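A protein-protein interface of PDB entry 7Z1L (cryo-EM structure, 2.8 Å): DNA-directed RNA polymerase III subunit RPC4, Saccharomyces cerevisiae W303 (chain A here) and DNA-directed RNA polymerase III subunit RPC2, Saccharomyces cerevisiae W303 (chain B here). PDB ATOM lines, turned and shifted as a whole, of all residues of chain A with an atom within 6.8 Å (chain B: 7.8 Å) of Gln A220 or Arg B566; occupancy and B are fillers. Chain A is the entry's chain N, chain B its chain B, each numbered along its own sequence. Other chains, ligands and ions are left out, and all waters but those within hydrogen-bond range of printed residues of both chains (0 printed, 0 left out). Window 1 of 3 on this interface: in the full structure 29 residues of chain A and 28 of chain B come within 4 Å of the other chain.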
ATOM      1  N   VAL A 215       8.011   1.180 -20.278  1.00  0.00           N
ATOM      2  CA  VAL A 215       9.088   0.357 -20.824  1.00  0.00           C
ATOM      3  C   VAL A 215      10.043   1.159 -21.698  1.00  0.00           C
ATOM      4  O   VAL A 215      11.114   0.653 -22.059  1.00  0.00           O
ATOM      5  CB  VAL A 215       8.459  -0.808 -21.617  1.00  0.00           C
ATOM      6  CG1 VAL A 215       7.776  -0.287 -22.876  1.00  0.00           C
ATOM      7  CG2 VAL A 215       9.455  -1.941 -21.903  1.00  0.00           C
ATOM      8  N   LYS A 216       9.696   2.409 -22.024  1.00  0.00           N
ATOM      9  CA  LYS A 216      10.493   3.198 -22.961  1.00  0.00           C
ATOM     10  C   LYS A 216      11.900   3.446 -22.432  1.00  0.00           C
ATOM     11  O   LYS A 216      12.864   3.469 -23.206  1.00  0.00           O
ATOM     12  CB  LYS A 216       9.788   4.521 -23.258  1.00  0.00           C
ATOM     13  CG  LYS A 216       8.846   4.459 -24.448  1.00  0.00           C
ATOM     14  CD  LYS A 216       7.840   5.596 -24.426  1.00  0.00           C
ATOM     15  CE  LYS A 216       6.968   5.580 -25.670  1.00  0.00           C
ATOM     16  NZ  LYS A 216       6.678   4.194 -26.126  1.00  0.00           N
ATOM     17  N   ARG A 217      12.037   3.626 -21.116  1.00  0.00           N
ATOM     18  CA  ARG A 217      13.363   3.732 -20.512  1.00  0.00           C
ATOM     19  C   ARG A 217      14.165   2.450 -20.710  1.00  0.00           C
ATOM     20  O   ARG A 217      15.319   2.492 -21.158  1.00  0.00           O
ATOM     21  CB  ARG A 217      13.226   4.049 -19.022  1.00  0.00           C
ATOM     22  CG  ARG A 217      14.537   4.148 -18.249  1.00  0.00           C
ATOM     23  CD  ARG A 217      15.342   5.390 -18.610  1.00  0.00           C
ATOM     24  NE  ARG A 217      16.192   5.207 -19.780  1.00  0.00           N
ATOM     25  CZ  ARG A 217      16.858   6.188 -20.373  1.00  0.00           C
ATOM     26  NH1 ARG A 217      16.804   7.428 -19.920  1.00  0.00           N
ATOM     27  NH2 ARG A 217      17.596   5.916 -21.445  1.00  0.00           N
ATOM     28  N   GLU A 218      13.560   1.302 -20.389  1.00  0.00           N
ATOM     29  CA  GLU A 218      14.254   0.023 -20.513  1.00  0.00           C
ATOM     30  C   GLU A 218      14.602  -0.286 -21.964  1.00  0.00           C
ATOM     31  O   GLU A 218      15.712  -0.743 -22.254  1.00  0.00           O
ATOM     32  CB  GLU A 218      13.400  -1.094 -19.915  1.00  0.00           C
ATOM     33  CG  GLU A 218      13.963  -2.491 -20.130  1.00  0.00           C
ATOM     34  CD  GLU A 218      13.193  -3.553 -19.372  1.00  0.00           C
ATOM     35  OE1 GLU A 218      12.163  -3.214 -18.753  1.00  0.00           O
ATOM     36  OE2 GLU A 218      13.619  -4.726 -19.393  1.00  0.00           O
ATOM     37  N   ILE A 219      13.673  -0.032 -22.887  1.00  0.00           N
ATOM     38  CA  ILE A 219      13.928  -0.297 -24.300  1.00  0.00           C
ATOM     39  C   ILE A 219      15.018   0.628 -24.833  1.00  0.00           C
ATOM     40  O   ILE A 219      15.916   0.194 -25.570  1.00  0.00           O
ATOM     41  CB  ILE A 219      12.619  -0.173 -25.102  1.00  0.00           C
ATOM     42  CG1 ILE A 219      11.749  -1.410 -24.882  1.00  0.00           C
ATOM     43  CG2 ILE A 219      12.895   0.012 -26.586  1.00  0.00           C
ATOM     44  CD1 ILE A 219      10.372  -1.302 -25.485  1.00  0.00           C
ATOM     45  N   GLN A 220      14.964   1.911 -24.462  1.00  0.00           N
ATOM     46  CA  GLN A 220      15.967   2.866 -24.925  1.00  0.00           C
ATOM     47  C   GLN A 220      17.353   2.517 -24.398  1.00  0.00           C
ATOM     48  O   GLN A 220      18.355   2.699 -25.100  1.00  0.00           O
ATOM     49  CB  GLN A 220      15.571   4.282 -24.506  1.00  0.00           C
ATOM     50  CG  GLN A 220      16.154   5.375 -25.385  1.00  0.00           C
ATOM     51  CD  GLN A 220      15.334   6.648 -25.349  1.00  0.00           C
ATOM     52  OE1 GLN A 220      14.550   6.869 -24.426  1.00  0.00           O
ATOM     53  NE2 GLN A 220      15.508   7.493 -26.357  1.00  0.00           N
ATOM     54  N   GLU A 221      17.435   2.015 -23.162  1.00  0.00           N
ATOM     55  CA  GLU A 221      18.733   1.588 -22.645  1.00  0.00           C
ATOM     56  C   GLU A 221      19.176   0.262 -23.255  1.00  0.00           C
ATOM     57  O   GLU A 221      20.379   0.013 -23.391  1.00  0.00           O
ATOM     58  CB  GLU A 221      18.688   1.486 -21.121  1.00  0.00           C
ATOM     59  CG  GLU A 221      18.660   2.830 -20.414  1.00  0.00           C
ATOM     60  CD  GLU A 221      18.287   2.712 -18.952  1.00  0.00           C
ATOM     61  OE1 GLU A 221      17.571   1.753 -18.595  1.00  0.00           O
ATOM     62  OE2 GLU A 221      18.709   3.579 -18.158  1.00  0.00           O
ATOM     63  N   ALA A 222      18.224  -0.598 -23.628  1.00  0.00           N
ATOM     64  CA  ALA A 222      18.578  -1.904 -24.172  1.00  0.00           C
ATOM     65  C   ALA A 222      19.047  -1.811 -25.616  1.00  0.00           C
ATOM     66  O   ALA A 222      19.816  -2.666 -26.070  1.00  0.00           O
ATOM     67  CB  ALA A 222      17.387  -2.858 -24.065  1.00  0.00           C
ATOM     68  N   LEU A 223      18.575  -0.808 -26.361  1.00  0.00           N
ATOM     69  CA  LEU A 223      19.015  -0.658 -27.748  1.00  0.00           C
ATOM     70  C   LEU A 223      20.511  -0.372 -27.830  1.00  0.00           C
ATOM     71  O   LEU A 223      21.212  -0.922 -28.687  1.00  0.00           O
ATOM     72  CB  LEU A 223      18.219   0.441 -28.453  1.00  0.00           C
ATOM     73  CG  LEU A 223      16.729   0.180 -28.659  1.00  0.00           C
ATOM     74  CD1 LEU A 223      16.052   1.405 -29.243  1.00  0.00           C
ATOM     75  CD2 LEU A 223      16.503  -1.048 -29.526  1.00  0.00           C
ATOM     76  N   SER A 224      21.017   0.498 -26.954  1.00  0.00           N
ATOM     77  CA  SER A 224      22.454   0.753 -26.921  1.00  0.00           C
ATOM     78  C   SER A 224      23.217  -0.460 -26.402  1.00  0.00           C
ATOM     79  O   SER A 224      24.171  -0.921 -27.039  1.00  0.00           O
ATOM     80  CB  SER A 224      22.751   1.983 -26.064  1.00  0.00           C
ATOM     81  OG  SER A 224      24.142   2.251 -26.029  1.00  0.00           O
ATOM     82  N   GLU A 225      22.799  -0.988 -25.248  1.00  0.00           N
ATOM     83  CA  GLU A 225      23.383  -2.177 -24.621  1.00  0.00           C
ATOM     84  C   GLU A 225      24.889  -2.004 -24.391  1.00  0.00           C
ATOM     85  O   GLU A 225      25.728  -2.648 -25.026  1.00  0.00           O
ATOM     86  CB  GLU A 225      23.074  -3.440 -25.435  1.00  0.00           C
ATOM     87  CG  GLU A 225      23.358  -4.743 -24.694  1.00  0.00           C
ATOM     88  CD  GLU A 225      22.660  -4.825 -23.347  1.00  0.00           C
ATOM     89  OE1 GLU A 225      21.491  -4.394 -23.244  1.00  0.00           O
ATOM     90  OE2 GLU A 225      23.282  -5.324 -22.386  1.00  0.00           O
ATOM     91  N   GLU A 279      14.517  15.009 -17.883  1.00  0.00           N
ATOM     92  CA  GLU A 279      15.438  15.295 -18.976  1.00  0.00           C
ATOM     93  C   GLU A 279      16.823  15.664 -18.468  1.00  0.00           C
ATOM     94  O   GLU A 279      17.809  15.410 -19.159  1.00  0.00           O
ATOM     95  CB  GLU A 279      14.893  16.412 -19.859  1.00  0.00           C
ATOM     96  CG  GLU A 279      13.647  16.036 -20.624  1.00  0.00           C
ATOM     97  CD  GLU A 279      13.139  17.175 -21.467  1.00  0.00           C
ATOM     98  OE1 GLU A 279      13.695  18.288 -21.354  1.00  0.00           O
ATOM     99  OE2 GLU A 279      12.178  16.964 -22.232  1.00  0.00           O
ATOM    100  N   LEU A 282      18.332  12.326 -17.854  1.00  0.00           N
ATOM    101  CA  LEU A 282      18.630  11.728 -19.150  1.00  0.00           C
ATOM    102  C   LEU A 282      19.850  12.380 -19.790  1.00  0.00           C
ATOM    103  O   LEU A 282      20.670  11.697 -20.410  1.00  0.00           O
ATOM    104  CB  LEU A 282      17.409  11.845 -20.064  1.00  0.00           C
ATOM    105  CG  LEU A 282      17.455  11.285 -21.489  1.00  0.00           C
ATOM    106  CD1 LEU A 282      18.171   9.947 -21.547  1.00  0.00           C
ATOM    107  CD2 LEU A 282      16.049  11.162 -22.055  1.00  0.00           C
ATOM    108  N   ASP A 286      23.275  10.600 -20.717  1.00  0.00           N
ATOM    109  CA  ASP A 286      23.739  10.702 -22.095  1.00  0.00           C
ATOM    110  C   ASP A 286      25.168  11.224 -22.156  1.00  0.00           C
ATOM    111  O   ASP A 286      25.964  10.758 -22.975  1.00  0.00           O
ATOM    112  CB  ASP A 286      22.807  11.617 -22.888  1.00  0.00           C
ATOM    113  CG  ASP A 286      21.649  10.868 -23.516  1.00  0.00           C
ATOM    114  OD1 ASP A 286      21.598   9.629 -23.384  1.00  0.00           O
ATOM    115  OD2 ASP A 286      20.789  11.522 -24.142  1.00  0.00           O
ATOM    116  N   GLY A 383      24.226  15.603 -27.040  1.00  0.00           N
ATOM    117  CA  GLY A 383      23.320  14.549 -26.619  1.00  0.00           C
ATOM    118  C   GLY A 383      23.304  13.422 -27.621  1.00  0.00           C
ATOM    119  O   GLY A 383      23.469  13.641 -28.821  1.00  0.00           O
ATOM    120  N   LYS A 384      23.078  12.202 -27.132  1.00  0.00           N
ATOM    121  CA  LYS A 384      23.223  11.060 -28.027  1.00  0.00           C
ATOM    122  C   LYS A 384      22.012  10.848 -28.930  1.00  0.00           C
ATOM    123  O   LYS A 384      22.059   9.965 -29.794  1.00  0.00           O
ATOM    124  CB  LYS A 384      23.527   9.789 -27.231  1.00  0.00           C
ATOM    125  CG  LYS A 384      22.333   9.110 -26.605  1.00  0.00           C
ATOM    126  CD  LYS A 384      22.770   7.880 -25.826  1.00  0.00           C
ATOM    127  CE  LYS A 384      23.428   6.858 -26.738  1.00  0.00           C
ATOM    128  NZ  LYS A 384      23.656   5.559 -26.050  1.00  0.00           N
ATOM    129  N   GLY A 385      20.941  11.619 -28.757  1.00  0.00           N
ATOM    130  CA  GLY A 385      19.886  11.668 -29.755  1.00  0.00           C
ATOM    131  C   GLY A 385      19.101  10.373 -29.930  1.00  0.00           C
ATOM    132  O   GLY A 385      18.960   9.555 -29.019  1.00  0.00           O
ATOM    133  N   ALA A 386      18.585  10.204 -31.145  1.00  0.00           N
ATOM    134  CA  ALA A 386      17.747   9.059 -31.465  1.00  0.00           C
ATOM    135  C   ALA A 386      18.556   7.767 -31.459  1.00  0.00           C
ATOM    136  O   ALA A 386      19.733   7.740 -31.828  1.00  0.00           O
ATOM    137  CB  ALA A 386      17.081   9.249 -32.826  1.00  0.00           C
ATOM    138  N   GLU A 387      17.907   6.687 -31.033  1.00  0.00           N
ATOM    139  CA  GLU A 387      18.520   5.366 -30.955  1.00  0.00           C
ATOM    140  C   GLU A 387      18.046   4.543 -32.144  1.00  0.00           C
ATOM    141  O   GLU A 387      16.858   4.221 -32.246  1.00  0.00           O
ATOM    142  CB  GLU A 387      18.167   4.676 -29.638  1.00  0.00           C
ATOM    143  CG  GLU A 387      18.512   5.487 -28.407  1.00  0.00           C
ATOM    144  CD  GLU A 387      19.994   5.778 -28.301  1.00  0.00           C
ATOM    145  OE1 GLU A 387      20.805   4.884 -28.620  1.00  0.00           O
ATOM    146  OE2 GLU A 387      20.347   6.906 -27.904  1.00  0.00           O
ATOM    147  N   ASN B 275       5.472  -0.218 -30.578  1.00  0.00           N
ATOM    148  CA  ASN B 275       5.626  -1.287 -29.603  1.00  0.00           C
ATOM    149  C   ASN B 275       4.326  -1.653 -28.900  1.00  0.00           C
ATOM    150  O   ASN B 275       4.310  -2.617 -28.128  1.00  0.00           O
ATOM    151  CB  ASN B 275       6.679  -0.896 -28.563  1.00  0.00           C
ATOM    152  CG  ASN B 275       8.073  -0.828 -29.148  1.00  0.00           C
ATOM    153  OD1 ASN B 275       8.305  -1.256 -30.279  1.00  0.00           O
ATOM    154  ND2 ASN B 275       9.009  -0.284 -28.383  1.00  0.00           N
ATOM    155  N   GLY B 537      18.492  20.832 -32.797  1.00  0.00           N
ATOM    156  CA  GLY B 537      18.718  19.470 -32.359  1.00  0.00           C
ATOM    157  C   GLY B 537      17.664  18.472 -32.786  1.00  0.00           C
ATOM    158  O   GLY B 537      17.488  17.437 -32.138  1.00  0.00           O
ATOM    159  N   VAL B 538      16.958  18.764 -33.871  1.00  0.00           N
ATOM    160  CA  VAL B 538      15.943  17.863 -34.400  1.00  0.00           C
ATOM    161  C   VAL B 538      16.592  16.974 -35.452  1.00  0.00           C
ATOM    162  O   VAL B 538      17.103  17.466 -36.463  1.00  0.00           O
ATOM    163  CB  VAL B 538      14.759  18.643 -34.990  1.00  0.00           C
ATOM    164  CG1 VAL B 538      13.863  17.725 -35.800  1.00  0.00           C
ATOM    165  CG2 VAL B 538      13.975  19.325 -33.886  1.00  0.00           C
ATOM    166  N   GLU B 539      16.580  15.666 -35.212  1.00  0.00           N
ATOM    167  CA  GLU B 539      17.086  14.725 -36.198  1.00  0.00           C
ATOM    168  C   GLU B 539      16.080  14.587 -37.333  1.00  0.00           C
ATOM    169  O   GLU B 539      14.884  14.388 -37.093  1.00  0.00           O
ATOM    170  CB  GLU B 539      17.360  13.367 -35.555  1.00  0.00           C
ATOM    171  CG  GLU B 539      18.470  13.378 -34.522  1.00  0.00           C
ATOM    172  CD  GLU B 539      17.946  13.515 -33.107  1.00  0.00           C
ATOM    173  OE1 GLU B 539      16.712  13.500 -32.925  1.00  0.00           O
ATOM    174  OE2 GLU B 539      18.768  13.640 -32.175  1.00  0.00           O
ATOM    175  N   SER B 548      12.149   2.885 -34.205  1.00  0.00           N
ATOM    176  CA  SER B 548      12.250   3.617 -32.952  1.00  0.00           C
ATOM    177  C   SER B 548      11.752   5.052 -33.069  1.00  0.00           C
ATOM    178  O   SER B 548      12.220   5.927 -32.333  1.00  0.00           O
ATOM    179  CB  SER B 548      13.694   3.604 -32.453  1.00  0.00           C
ATOM    180  OG  SER B 548      14.426   4.691 -32.991  1.00  0.00           O
ATOM    181  N   LEU B 551       9.658   5.994 -29.836  1.00  0.00           N
ATOM    182  CA  LEU B 551      10.310   5.949 -28.535  1.00  0.00           C
ATOM    183  C   LEU B 551      10.647   7.333 -28.003  1.00  0.00           C
ATOM    184  O   LEU B 551      11.066   7.451 -26.848  1.00  0.00           O
ATOM    185  CB  LEU B 551      11.581   5.104 -28.611  1.00  0.00           C
ATOM    186  CG  LEU B 551      11.368   3.621 -28.909  1.00  0.00           C
ATOM    187  CD1 LEU B 551      12.696   2.899 -28.964  1.00  0.00           C
ATOM    188  CD2 LEU B 551      10.461   2.996 -27.863  1.00  0.00           C
ATOM    189  N   ASN B 552      10.471   8.372 -28.814  1.00  0.00           N
ATOM    190  CA  ASN B 552      10.777   9.735 -28.411  1.00  0.00           C
ATOM    191  C   ASN B 552       9.833  10.696 -29.122  1.00  0.00           C
ATOM    192  O   ASN B 552       9.103  10.313 -30.039  1.00  0.00           O
ATOM    193  CB  ASN B 552      12.260  10.063 -28.657  1.00  0.00           C
ATOM    194  CG  ASN B 552      12.659  10.008 -30.131  1.00  0.00           C
ATOM    195  OD1 ASN B 552      11.830   9.842 -31.026  1.00  0.00           O
ATOM    196  ND2 ASN B 552      13.956  10.137 -30.382  1.00  0.00           N
ATOM    197  N   TYR B 553       9.852  11.950 -28.678  1.00  0.00           N
ATOM    198  CA  TYR B 553       8.918  12.942 -29.195  1.00  0.00           C
ATOM    199  C   TYR B 553       9.231  13.296 -30.643  1.00  0.00           C
ATOM    200  O   TYR B 553      10.394  13.377 -31.046  1.00  0.00           O
ATOM    201  CB  TYR B 553       8.959  14.204 -28.333  1.00  0.00           C
ATOM    202  CG  TYR B 553       8.063  14.159 -27.119  1.00  0.00           C
ATOM    203  CD1 TYR B 553       8.286  13.250 -26.097  1.00  0.00           C
ATOM    204  CD2 TYR B 553       6.995  15.036 -26.993  1.00  0.00           C
ATOM    205  CE1 TYR B 553       7.469  13.212 -24.984  1.00  0.00           C
ATOM    206  CE2 TYR B 553       6.173  15.006 -25.887  1.00  0.00           C
ATOM    207  CZ  TYR B 553       6.414  14.092 -24.885  1.00  0.00           C
ATOM    208  OH  TYR B 553       5.596  14.060 -23.781  1.00  0.00           O
ATOM    209  N   GLY B 554       8.177  13.505 -31.428  1.00  0.00           N
ATOM    210  CA  GLY B 554       8.307  14.000 -32.778  1.00  0.00           C
ATOM    211  C   GLY B 554       8.069  15.496 -32.837  1.00  0.00           C
ATOM    212  O   GLY B 554       7.541  16.095 -31.905  1.00  0.00           O
ATOM    213  N   VAL B 555       8.484  16.103 -33.945  1.00  0.00           N
ATOM    214  CA  VAL B 555       8.303  17.530 -34.178  1.00  0.00           C
ATOM    215  C   VAL B 555       7.447  17.698 -35.424  1.00  0.00           C
ATOM    216  O   VAL B 555       7.717  17.075 -36.457  1.00  0.00           O
ATOM    217  CB  VAL B 555       9.647  18.263 -34.337  1.00  0.00           C
ATOM    218  CG1 VAL B 555       9.438  19.766 -34.306  1.00  0.00           C
ATOM    219  CG2 VAL B 555      10.618  17.840 -33.261  1.00  0.00           C
ATOM    220  N   SER B 564      12.541  14.149 -35.361  1.00  0.00           N
ATOM    221  CA  SER B 564      12.409  13.691 -33.987  1.00  0.00           C
ATOM    222  C   SER B 564      13.311  14.509 -33.074  1.00  0.00           C
ATOM    223  O   SER B 564      14.353  15.018 -33.496  1.00  0.00           O
ATOM    224  CB  SER B 564      12.754  12.205 -33.859  1.00  0.00           C
ATOM    225  OG  SER B 564      14.150  11.995 -33.975  1.00  0.00           O
ATOM    226  N   ILE B 565      12.901  14.638 -31.815  1.00  0.00           N
ATOM    227  CA  ILE B 565      13.643  15.404 -30.822  1.00  0.00           C
ATOM    228  C   ILE B 565      13.852  14.528 -29.593  1.00  0.00           C
ATOM    229  O   ILE B 565      12.928  13.839 -29.148  1.00  0.00           O
ATOM    230  CB  ILE B 565      12.927  16.725 -30.464  1.00  0.00           C
ATOM    231  CG1 ILE B 565      13.736  17.527 -29.443  1.00  0.00           C
ATOM    232  CG2 ILE B 565      11.498  16.488 -29.983  1.00  0.00           C
ATOM    233  CD1 ILE B 565      15.046  18.044 -29.983  1.00  0.00           C
ATOM    234  N   ARG B 566      15.084  14.511 -29.079  1.00  0.00           N
ATOM    235  CA  ARG B 566      15.365  13.716 -27.887  1.00  0.00           C
ATOM    236  C   ARG B 566      14.811  14.379 -26.633  1.00  0.00           C
ATOM    237  O   ARG B 566      14.206  13.711 -25.787  1.00  0.00           O
ATOM    238  CB  ARG B 566      16.870  13.487 -27.752  1.00  0.00           C
ATOM    239  CG  ARG B 566      17.268  12.718 -26.503  1.00  0.00           C
ATOM    240  CD  ARG B 566      16.616  11.345 -26.471  1.00  0.00           C
ATOM    241  NE  ARG B 566      17.224  10.462 -25.483  1.00  0.00           N
ATOM    242  CZ  ARG B 566      18.373   9.821 -25.653  1.00  0.00           C
ATOM    243  NH1 ARG B 566      19.082   9.957 -26.759  1.00  0.00           N
ATOM    244  NH2 ARG B 566      18.820   9.024 -24.689  1.00  0.00           N
ATOM    245  N   PHE B 567      14.998  15.691 -26.498  1.00  0.00           N
ATOM    246  CA  PHE B 567      14.538  16.430 -25.324  1.00  0.00           C
ATOM    247  C   PHE B 567      13.472  17.431 -25.744  1.00  0.00           C
ATOM    248  O   PHE B 567      13.804  18.518 -26.239  1.00  0.00           O
ATOM    249  CB  PHE B 567      15.707  17.147 -24.644  1.00  0.00           C
ATOM    250  CG  PHE B 567      16.914  16.279 -24.433  1.00  0.00           C
ATOM    251  CD1 PHE B 567      16.993  15.435 -23.340  1.00  0.00           C
ATOM    252  CD2 PHE B 567      17.971  16.312 -25.327  1.00  0.00           C
ATOM    253  CE1 PHE B 567      18.102  14.637 -23.145  1.00  0.00           C
ATOM    254  CE2 PHE B 567      19.083  15.515 -25.136  1.00  0.00           C
ATOM    255  CZ  PHE B 567      19.147  14.676 -24.043  1.00  0.00           C
ATOM    256  N   PRO B 568      12.184  17.120 -25.573  1.00  0.00           N
ATOM    257  CA  PRO B 568      11.152  18.059 -26.037  1.00  0.00           C
ATOM    258  C   PRO B 568      11.021  19.305 -25.179  1.00  0.00           C
ATOM    259  O   PRO B 568      10.794  20.392 -25.723  1.00  0.00           O
ATOM    260  CB  PRO B 568       9.874  17.208 -26.005  1.00  0.00           C
ATOM    261  CG  PRO B 568      10.158  16.146 -25.000  1.00  0.00           C
ATOM    262  CD  PRO B 568      11.611  15.828 -25.161  1.00  0.00           C
ATOM    263  N   THR B 569      11.146  19.182 -23.854  1.00  0.00           N
ATOM    264  CA  THR B 569      10.951  20.341 -22.986  1.00  0.00           C
ATOM    265  C   THR B 569      12.049  21.379 -23.185  1.00  0.00           C
ATOM    266  O   THR B 569      11.770  22.584 -23.220  1.00  0.00           O
ATOM    267  CB  THR B 569      10.882  19.903 -21.523  1.00  0.00           C
ATOM    268  OG1 THR B 569       9.890  18.881 -21.376  1.00  0.00           O
ATOM    269  CG2 THR B 569      10.521  21.075 -20.629  1.00  0.00           C
ATOM    270  N   LYS B 570      13.300  20.935 -23.328  1.00  0.00           N
ATOM    271  CA  LYS B 570      14.390  21.871 -23.581  1.00  0.00           C
ATOM    272  C   LYS B 570      14.236  22.545 -24.938  1.00  0.00           C
ATOM    273  O   LYS B 570      14.508  23.743 -25.077  1.00  0.00           O
ATOM    274  CB  LYS B 570      15.735  21.153 -23.490  1.00  0.00           C
ATOM    275  CG  LYS B 570      16.928  22.091 -23.458  1.00  0.00           C
ATOM    276  CD  LYS B 570      18.218  21.353 -23.760  1.00  0.00           C
ATOM    277  CE  LYS B 570      18.517  20.314 -22.693  1.00  0.00           C
ATOM    278  NZ  LYS B 570      19.347  19.201 -23.227  1.00  0.00           N
ATOM    279  N   PHE B 571      13.798  21.790 -25.950  1.00  0.00           N
ATOM    280  CA  PHE B 571      13.555  22.365 -27.269  1.00  0.00           C
ATOM    281  C   PHE B 571      12.457  23.420 -27.220  1.00  0.00           C
ATOM    282  O   PHE B 571      12.591  24.498 -27.813  1.00  0.00           O
ATOM    283  CB  PHE B 571      13.195  21.251 -28.251  1.00  0.00           C
ATOM    284  CG  PHE B 571      12.860  21.731 -29.632  1.00  0.00           C
ATOM    285  CD1 PHE B 571      13.862  22.048 -30.529  1.00  0.00           C
ATOM    286  CD2 PHE B 571      11.543  21.837 -30.043  1.00  0.00           C
ATOM    287  CE1 PHE B 571      13.558  22.480 -31.801  1.00  0.00           C
ATOM    288  CE2 PHE B 571      11.233  22.269 -31.315  1.00  0.00           C
ATOM    289  CZ  PHE B 571      12.242  22.590 -32.195  1.00  0.00           C
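The side-chain carboxylate (OE2) of Glu A279 lies within hydrogen-bond range of the backbone NH (N) of Thr B569 (2.9 Å). The backbone NH (N) of Lys B570 lies within hydrogen-bond range of the side-chain carboxylate (OE1) of Glu A279 (3.3 Å). The side-chain carboxylate (OD1) of Asp A286 lies within salt-bridge range of the guanidinium group (NH2) of Arg B566. The side-chain hydroxyl (OG) of Ser B548 lies within hydrogen-bond range of the backbone carbonyl oxygen (O) of Glu A387 (2.6 Å). NH1 of Arg B566 is in salt-bridge range of OE2 of Glu A387 (3.5 Å). The side-chain carboxylate (OE2) of Glu A279 lies close to the backbone nitrogen (N) of Pro B568. The backbone carbonyl oxygen (O) of Gly A385 lies close to the guanidinium group (NH1) of Arg B566 (2.3 Å).
The side-chain amino group of Lys A384 is in hydrogen-bond range of the side-chain hydroxyl of Ser A224 (3.3 Å). The side-chain amino group (NZ) of Lys A384 lies within salt-bridge range of the side-chain carboxylate (OE1) of Glu A387 (3.9 Å). O of Ser B564 is in hydrogen-bond range of N of Glu B539, at 2.9 Å.
Among the printed residues, merely in contact across the chains: Ile A219 with Asn B275 (3.4 Å), Ile A219 with Leu B551 (3.7 Å), Gln A220 with Arg B566 (3.5 Å), Leu A223 with Leu B551 (3.7 Å), Glu A279 with Phe B567 (3.8 Å), Leu A282 with Arg B566 (3.3 Å), Leu A282 with Phe B567 (3.8 Å), Asp A286 with Phe B567 (3.6 Å), Lys A384 with Arg B566 (3.4 Å), Gly A385 with Glu B539 (3.3 Å) and Ala A386 with Glu B539 (3.6 Å).
Of chain A, only Gln A220, Leu A282, Asp A286, Lys A384, Gly A385 and Glu A387 come within 4 Å of Arg B566. Printed residues of chain B within 4 Å of Gly A385: Glu B539 (3.3 Å) and Arg B566 (2.3 Å). Printed residues of chain B within 4 Å of Leu A223: Leu B551. Of the printed residues of chain A, Ser B548 touches Glu A387 (2.6 Å). Printed residues of chain B within 4 Å of Asp A286: Arg B566 and Phe B567. Gly A383 touches none of the printed residues of chain B. Gly B537 touches none of the printed residues of chain A. The nearest residue of chain A that does not touch Arg B566 is Ala A386 (4.4 Å).
Of the 18 printed residues of chain B, 9 touch a printed residue of chain A. Of the 19 printed residues of chain A, 10 touch a printed residue of chain B.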
